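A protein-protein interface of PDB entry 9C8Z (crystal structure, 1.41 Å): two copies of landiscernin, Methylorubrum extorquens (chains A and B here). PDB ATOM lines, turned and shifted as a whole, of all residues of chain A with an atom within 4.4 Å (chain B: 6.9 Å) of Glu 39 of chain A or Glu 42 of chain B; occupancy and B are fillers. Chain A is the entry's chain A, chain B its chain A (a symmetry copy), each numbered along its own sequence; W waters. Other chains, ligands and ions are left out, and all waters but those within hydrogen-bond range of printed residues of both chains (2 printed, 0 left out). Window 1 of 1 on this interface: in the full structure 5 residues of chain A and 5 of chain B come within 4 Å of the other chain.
Water W1 bridges the backbone carbonyl oxygen of Glu 42 of chain B (2.7 Å) and the guanidinium group of Arg 38 of chain A (2.9 Å).
Water W2 lies within hydrogen-bond range of the backbone carbonyl oxygen of Glu 42 of chain A (2.7 Å) and the guanidinium group of Arg 38 of chain B (2.9 Å).
Glu 39 of chain A touches Glu 42 of chain B, and with the chains exchanged Glu 42 of chain A touches Glu 39 of chain B.
Glu 42 of chain B touches its own counterpart, Glu 42 of chain A.
Glu 44 of chain B touches its own counterpart, Glu 44 of chain A.
Glu 44 of chain A touches Glu 47 of chain B, and with the chains exchanged Glu 47 of chain A touches Glu 44 of chain B.
Positions printed for both chains: 36, 37, 38, 39, 40, 41, 42, 43, 44 and 47.
Along chain A the printed residues that touch a printed residue of chain B span positions 38 to 47.
Of the 11 printed residues of chain B, 5 touch a printed residue of chain A.
Among the printed residues, 10 pairs touch across the chains.
Among the printed residues, Asp or Glu carboxylates within 4 Å of a Lys or Arg side-chain nitrogen of the other chain: Arg 38 of chain A with Glu 42 of chain B and Glu 42 of chain A with Arg 38 of chain B.
Glu 39 of chain A touches just these residues of chain B: Glu 42 (3.1 Å) and Glu 44 (3.1 Å).
Printed residues of chain B within 4 Å of Glu 42 of chain A: Arg 38, Glu 39 and Glu 42.
Printed residues of chain A within 4 Å of Glu 39 of chain B: Glu 42 and Glu 44.
Glu 42 of chain B touches just these residues of chain A: Arg 38 (3.4 Å), Glu 39 (3.1 Å) and Glu 42 (2.4 Å).
Of the printed residues of chain A, Glu 44 of chain B touches Glu 39 (3.1 Å), Glu 44 (3.96 Å) and Glu 47 (2.6 Å).
Of the printed residues of chain A, Glu 47 of chain B touches Glu 44 (2.6 Å).
The nearest residue of chain B that does not touch Glu 39 of chain A is Glu 39 of chain B (4.8 Å).
Among the printed residues, merely in contact across the chains: Glu 44 of chain A with Glu 44 of chain B.
NE of Arg 38 of chain A is in salt-bridge range of OE2 of Glu 42 of chain B, at 3.4 Å.
The side-chain carboxylate (OE2) of Glu 42 of chain A is in salt-bridge range of the guanidinium group (NE) of Arg 38 of chain B, at 3.4 Å.
The side-chain carboxylate (OE1) of Glu 44 of chain A lies close to the side-chain carboxylate (OE2) of Glu 47 of chain B.
OE2 of Glu 47 of chain A lies close to OE1 of Glu 44 of chain B, 2.6 Å away.
OE1 of Glu 42 of chain B lies close to OE2 of Glu 39 of chain A, at 3.1 Å.
OE2 of Glu 44 of chain B lies close to OE2 of Glu 39 of chain A (3.1 Å).
OE2 of Glu 39 of chain B lies close to OE1 of Glu 42 of chain A, at 3.1 Å.
The side-chain carboxylate of Glu 42 of chain A lies close to the side-chain carboxylate of Glu 42 of chain B.
OE2 of Glu 39 of chain B lies close to OE2 of Glu 44 of chain A, at 3.1 Å.
The guanidinium group (NH2) of Arg 38 of chain A lies close to the side-chain carboxylate (OE2) of Glu 39 of chain A (2.9 Å).
NE of Arg 38 of chain A lies within salt-bridge range of OE2 of Glu 42 of chain A (3.98 Å).
NH2 of Arg 38 of chain B sits close to OE2 of Glu 39 of chain B (2.9 Å).
NE of Arg 38 of chain B is in salt-bridge range of OE2 of Glu 42 of chain B, at 3.98 Å.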
ATOM      1  N   ILE A  35       3.022   3.145  23.378  1.00  0.00           N
ATOM      2  CA  ILE A  35       3.617   4.466  23.172  1.00  0.00           C
ATOM      3  C   ILE A  35       4.573   4.810  24.307  1.00  0.00           C
ATOM      4  O   ILE A  35       5.686   5.304  24.075  1.00  0.00           O
ATOM      5  CB  ILE A  35       2.537   5.543  22.981  1.00  0.00           C
ATOM      6  CG1 ILE A  35       1.729   5.259  21.714  1.00  0.00           C
ATOM      7  CG2 ILE A  35       3.193   6.914  22.865  1.00  0.00           C
ATOM      8  CD1 ILE A  35       2.509   5.568  20.442  1.00  0.00           C
ATOM      9  N   ALA A  36       4.171   4.551  25.552  1.00  0.00           N
ATOM     10  CA  ALA A  36       5.067   4.829  26.666  1.00  0.00           C
ATOM     11  C   ALA A  36       6.358   4.030  26.524  1.00  0.00           C
ATOM     12  O   ALA A  36       7.452   4.562  26.722  1.00  0.00           O
ATOM     13  CB  ALA A  36       4.368   4.513  27.985  1.00  0.00           C
ATOM     14  N   GLU A  37       6.253   2.761  26.122  1.00  0.00           N
ATOM     15  CA  GLU A  37       7.451   1.940  25.944  1.00  0.00           C
ATOM     16  C   GLU A  37       8.317   2.439  24.797  1.00  0.00           C
ATOM     17  O   GLU A  37       9.552   2.429  24.899  1.00  0.00           O
ATOM     18  CB  GLU A  37       7.063   0.478  25.745  1.00  0.00           C
ATOM     19  CG  GLU A  37       6.433  -0.096  26.983  1.00  0.00           C
ATOM     20  CD  GLU A  37       5.700  -1.396  26.762  1.00  0.00           C
ATOM     21  OE1 GLU A  37       5.467  -1.796  25.610  1.00  0.00           O
ATOM     22  OE2 GLU A  37       5.305  -2.002  27.792  1.00  0.00           O
ATOM     23  N   ARG A  38       7.692   2.873  23.699  1.00  0.00           N
ATOM     24  CA  ARG A  38       8.462   3.440  22.599  1.00  0.00           C
ATOM     25  C   ARG A  38       9.229   4.671  23.059  1.00  0.00           C
ATOM     26  O   ARG A  38      10.427   4.811  22.795  1.00  0.00           O
ATOM     27  CB  ARG A  38       7.544   3.845  21.462  1.00  0.00           C
ATOM     28  CG  ARG A  38       8.312   4.454  20.292  1.00  0.00           C
ATOM     29  CD  ARG A  38       7.373   5.049  19.264  1.00  0.00           C
ATOM     30  NE  ARG A  38       6.772   6.269  19.784  1.00  0.00           N
ATOM     31  CZ  ARG A  38       5.700   6.855  19.273  1.00  0.00           C
ATOM     32  NH1 ARG A  38       5.059   6.337  18.234  1.00  0.00           N
ATOM     33  NH2 ARG A  38       5.256   7.981  19.824  1.00  0.00           N
ATOM     34  N   GLU A  39       8.548   5.579  23.755  1.00  0.00           N
ATOM     35  CA  GLU A  39       9.199   6.798  24.216  1.00  0.00           C
ATOM     36  C   GLU A  39      10.286   6.478  25.230  1.00  0.00           C
ATOM     37  O   GLU A  39      11.354   7.094  25.201  1.00  0.00           O
ATOM     38  CB  GLU A  39       8.156   7.783  24.753  1.00  0.00           C
ATOM     39  CG  GLU A  39       7.212   8.250  23.649  1.00  0.00           C
ATOM     40  CD  GLU A  39       7.958   8.901  22.480  1.00  0.00           C
ATOM     41  OE1 GLU A  39       8.866   9.728  22.742  1.00  0.00           O
ATOM     42  OE2 GLU A  39       7.679   8.590  21.301  1.00  0.00           O
ATOM     43  N   GLN A  40      10.056   5.486  26.109  1.00  0.00           N
ATOM     44  CA  GLN A  40      11.107   5.056  27.031  1.00  0.00           C
ATOM     45  C   GLN A  40      12.348   4.609  26.268  1.00  0.00           C
ATOM     46  O   GLN A  40      13.471   5.001  26.601  1.00  0.00           O
ATOM     47  CB  GLN A  40      10.577   3.906  27.878  1.00  0.00           C
ATOM     48  CG  GLN A  40      11.598   3.344  28.858  1.00  0.00           C
ATOM     49  CD  GLN A  40      11.132   2.035  29.498  1.00  0.00           C
ATOM     50  OE1 GLN A  40      10.626   1.136  28.811  1.00  0.00           O
ATOM     51  NE2 GLN A  40      11.260   1.941  30.818  1.00  0.00           N
ATOM     52  N   GLY A  41      12.158   3.787  25.233  1.00  0.00           N
ATOM     53  CA  GLY A  41      13.278   3.314  24.445  1.00  0.00           C
ATOM     54  C   GLY A  41      13.996   4.420  23.708  1.00  0.00           C
ATOM     55  O   GLY A  41      15.205   4.323  23.455  1.00  0.00           O
ATOM     56  N   GLU A  42      13.271   5.485  23.349  1.00  0.00           N
ATOM     57  CA  GLU A  42      13.873   6.654  22.718  1.00  0.00           C
ATOM     58  C   GLU A  42      14.586   7.545  23.720  1.00  0.00           C
ATOM     59  O   GLU A  42      15.265   8.505  23.321  1.00  0.00           O
ATOM     60  CB  GLU A  42      12.814   7.441  21.934  1.00  0.00           C
ATOM     61  CG  GLU A  42      12.228   6.637  20.796  1.00  0.00           C
ATOM     62  CD  GLU A  42      11.116   7.323  20.056  1.00  0.00           C
ATOM     63  OE1 GLU A  42      10.707   8.430  20.475  1.00  0.00           O
ATOM     64  OE2 GLU A  42      10.658   6.737  19.056  1.00  0.00           O
ATOM     65  N   GLY A  43      14.481   7.235  25.009  1.00  0.00           N
ATOM     66  CA  GLY A  43      15.021   8.128  26.011  1.00  0.00           C
ATOM     67  C   GLY A  43      14.167   9.334  26.311  1.00  0.00           C
ATOM     68  O   GLY A  43      14.640  10.250  26.991  1.00  0.00           O
ATOM     69  N   GLU A  44      12.920   9.364  25.827  1.00  0.00           N
ATOM     70  CA  GLU A  44      11.992  10.446  26.129  1.00  0.00           C
ATOM     71  C   GLU A  44      11.147  10.044  27.337  1.00  0.00           C
ATOM     72  O   GLU A  44       9.948   9.760  27.242  1.00  0.00           O
ATOM     73  CB  GLU A  44      11.147  10.754  24.904  1.00  0.00           C
ATOM     74  CG  GLU A  44      11.987  10.987  23.668  1.00  0.00           C
ATOM     75  CD  GLU A  44      11.304  11.900  22.722  1.00  0.00           C
ATOM     76  OE1 GLU A  44      11.021  13.016  23.170  1.00  0.00           O
ATOM     77  OE2 GLU A  44      11.009  11.505  21.565  1.00  0.00           O
ATOM     78  N   GLU A  47       8.047  12.016  28.094  1.00  0.00           N
ATOM     79  CA  GLU A  47       6.949  11.647  27.197  1.00  0.00           C
ATOM     80  C   GLU A  47       6.340  10.309  27.596  1.00  0.00           C
ATOM     81  O   GLU A  47       5.133  10.080  27.441  1.00  0.00           O
ATOM     82  CB  GLU A  47       7.518  11.509  25.787  1.00  0.00           C
ATOM     83  CG  GLU A  47       8.120  12.779  25.236  1.00  0.00           C
ATOM     84  CD  GLU A  47       7.050  13.774  24.943  1.00  0.00           C
ATOM     85  OE1 GLU A  47       6.641  14.512  25.859  1.00  0.00           O
ATOM     86  OE2 GLU A  47       6.569  13.768  23.796  1.00  0.00           O
ATOM     87  N   CYS A  48       7.179   9.400  28.065  1.00  0.00           N
ATOM     88  CA  CYS A  48       6.687   8.131  28.574  1.00  0.00           C
ATOM     89  C   CYS A  48       5.702   8.358  29.715  1.00  0.00           C
ATOM     90  O   CYS A  48       4.640   7.727  29.759  1.00  0.00           O
ATOM     91  CB  CYS A  48       7.892   7.323  29.047  1.00  0.00           C
ATOM     92  SG  CYS A  48       7.506   6.001  30.159  1.00  0.00           S
ATOM     93  N   ALA B  36      14.765  13.875  13.656  1.00  0.00           N
ATOM     94  CA  ALA B  36      13.676  14.771  13.290  1.00  0.00           C
ATOM     95  C   ALA B  36      12.639  14.032  12.452  1.00  0.00           C
ATOM     96  O   ALA B  36      11.435  14.166  12.679  1.00  0.00           O
ATOM     97  CB  ALA B  36      14.228  15.979  12.539  1.00  0.00           C
ATOM     98  N   GLU B  37      13.090  13.196  11.513  1.00  0.00           N
ATOM     99  CA  GLU B  37      12.152  12.438  10.684  1.00  0.00           C
ATOM    100  C   GLU B  37      11.372  11.416  11.498  1.00  0.00           C
ATOM    101  O   GLU B  37      10.172  11.219  11.264  1.00  0.00           O
ATOM    102  CB  GLU B  37      12.891  11.772   9.527  1.00  0.00           C
ATOM    103  CG  GLU B  37      13.447  12.790   8.572  1.00  0.00           C
ATOM    104  CD  GLU B  37      14.484  12.249   7.620  1.00  0.00           C
ATOM    105  OE1 GLU B  37      14.969  11.119   7.797  1.00  0.00           O
ATOM    106  OE2 GLU B  37      14.853  13.015   6.693  1.00  0.00           O
ATOM    107  N   ARG B  38      12.034  10.755  12.451  1.00  0.00           N
ATOM    108  CA  ARG B  38      11.325   9.824  13.320  1.00  0.00           C
ATOM    109  C   ARG B  38      10.237  10.544  14.102  1.00  0.00           C
ATOM    110  O   ARG B  38       9.090  10.089  14.166  1.00  0.00           O
ATOM    111  CB  ARG B  38      12.281   9.185  14.307  1.00  0.00           C
ATOM    112  CG  ARG B  38      11.573   8.208  15.243  1.00  0.00           C
ATOM    113  CD  ARG B  38      12.491   7.745  16.356  1.00  0.00           C
ATOM    114  NE  ARG B  38      12.712   8.829  17.303  1.00  0.00           N
ATOM    115  CZ  ARG B  38      13.684   8.853  18.203  1.00  0.00           C
ATOM    116  NH1 ARG B  38      14.572   7.871  18.285  1.00  0.00           N
ATOM    117  NH2 ARG B  38      13.772   9.890  19.030  1.00  0.00           N
ATOM    118  N   GLU B  39      10.580  11.679  14.708  1.00  0.00           N
ATOM    119  CA  GLU B  39       9.607  12.421  15.497  1.00  0.00           C
ATOM    120  C   GLU B  39       8.486  12.947  14.614  1.00  0.00           C
ATOM    121  O   GLU B  39       7.321  12.919  15.018  1.00  0.00           O
ATOM    122  CB  GLU B  39      10.306  13.528  16.293  1.00  0.00           C
ATOM    123  CG  GLU B  39      11.268  12.948  17.325  1.00  0.00           C
ATOM    124  CD  GLU B  39      10.572  11.995  18.301  1.00  0.00           C
ATOM    125  OE1 GLU B  39       9.469  12.345  18.790  1.00  0.00           O
ATOM    126  OE2 GLU B  39      11.084  10.887  18.576  1.00  0.00           O
ATOM    127  N   GLN B  40       8.806  13.388  13.384  1.00  0.00           N
ATOM    128  CA  GLN B  40       7.760  13.796  12.448  1.00  0.00           C
ATOM    129  C   GLN B  40       6.780  12.656  12.200  1.00  0.00           C
ATOM    130  O   GLN B  40       5.560  12.849  12.239  1.00  0.00           O
ATOM    131  CB  GLN B  40       8.409  14.216  11.136  1.00  0.00           C
ATOM    132  CG  GLN B  40       7.413  14.631  10.062  1.00  0.00           C
ATOM    133  CD  GLN B  40       8.068  14.789   8.689  1.00  0.00           C
ATOM    134  OE1 GLN B  40       8.862  13.939   8.261  1.00  0.00           O
ATOM    135  NE2 GLN B  40       7.773  15.897   8.015  1.00  0.00           N
ATOM    136  N   GLY B  41       7.303  11.455  11.945  1.00  0.00           N
ATOM    137  CA  GLY B  41       6.450  10.309  11.702  1.00  0.00           C
ATOM    138  C   GLY B  41       5.613   9.926  12.900  1.00  0.00           C
ATOM    139  O   GLY B  41       4.509   9.385  12.746  1.00  0.00           O
ATOM    140  N   GLU B  42       6.117  10.195  14.109  1.00  0.00           N
ATOM    141  CA  GLU B  42       5.363   9.957  15.334  1.00  0.00           C
ATOM    142  C   GLU B  42       4.324  11.037  15.587  1.00  0.00           C
ATOM    143  O   GLU B  42       3.509  10.906  16.515  1.00  0.00           O
ATOM    144  CB  GLU B  42       6.315   9.815  16.529  1.00  0.00           C
ATOM    145  CG  GLU B  42       7.230   8.620  16.393  1.00  0.00           C
ATOM    146  CD  GLU B  42       8.251   8.489  17.485  1.00  0.00           C
ATOM    147  OE1 GLU B  42       8.329   9.393  18.348  1.00  0.00           O
ATOM    148  OE2 GLU B  42       8.973   7.473  17.465  1.00  0.00           O
ATOM    149  N   GLY B  43       4.308  12.085  14.768  1.00  0.00           N
ATOM    150  CA  GLY B  43       3.437  13.205  15.049  1.00  0.00           C
ATOM    151  C   GLY B  43       3.937  14.145  16.116  1.00  0.00           C
ATOM    152  O   GLY B  43       3.172  15.003  16.567  1.00  0.00           O
ATOM    153  N   GLU B  44       5.201  14.013  16.536  1.00  0.00           N
ATOM    154  CA  GLU B  44       5.801  14.923  17.503  1.00  0.00           C
ATOM    155  C   GLU B  44       6.530  16.032  16.745  1.00  0.00           C
ATOM    156  O   GLU B  44       7.762  16.111  16.709  1.00  0.00           O
ATOM    157  CB  GLU B  44       6.722  14.149  18.431  1.00  0.00           C
ATOM    158  CG  GLU B  44       6.041  12.949  19.050  1.00  0.00           C
ATOM    159  CD  GLU B  44       6.628  12.627  20.373  1.00  0.00           C
ATOM    160  OE1 GLU B  44       6.578  13.531  21.212  1.00  0.00           O
ATOM    161  OE2 GLU B  44       7.172  11.509  20.566  1.00  0.00           O
ATOM    162  N   PHE B  45       5.725  16.895  16.109  1.00  0.00           N
ATOM    163  CA  PHE B  45       6.294  17.872  15.190  1.00  0.00           C
ATOM    164  C   PHE B  45       7.096  18.913  15.942  1.00  0.00           C
ATOM    165  O   PHE B  45       8.065  19.461  15.403  1.00  0.00           O
ATOM    166  CB  PHE B  45       5.171  18.533  14.410  1.00  0.00           C
ATOM    167  CG  PHE B  45       4.307  17.555  13.696  1.00  0.00           C
ATOM    168  CD1 PHE B  45       4.817  16.837  12.637  1.00  0.00           C
ATOM    169  CD2 PHE B  45       2.996  17.337  14.101  1.00  0.00           C
ATOM    170  CE1 PHE B  45       4.041  15.913  11.964  1.00  0.00           C
ATOM    171  CE2 PHE B  45       2.214  16.410  13.442  1.00  0.00           C
ATOM    172  CZ  PHE B  45       2.734  15.702  12.367  1.00  0.00           C
ATOM    173  N   GLU B  47       8.948  18.198  18.625  1.00  0.00           N
ATOM    174  CA  GLU B  47      10.221  17.507  18.846  1.00  0.00           C
ATOM    175  C   GLU B  47      11.056  17.473  17.573  1.00  0.00           C
ATOM    176  O   GLU B  47      12.292  17.522  17.613  1.00  0.00           O
ATOM    177  CB  GLU B  47       9.912  16.067  19.251  1.00  0.00           C
ATOM    178  CG  GLU B  47       9.121  15.942  20.531  1.00  0.00           C
ATOM    179  CD  GLU B  47       9.965  16.320  21.700  1.00  0.00           C
ATOM    180  OE1 GLU B  47      10.054  17.521  22.019  1.00  0.00           O
ATOM    181  OE2 GLU B  47      10.596  15.409  22.262  1.00  0.00           O
HETATM  182  O   HOH W   1       3.047   8.807  18.106  1.00  0.00           O
HETATM  183  O   HOH W   2      15.959   9.197  20.832  1.00  0.00           O
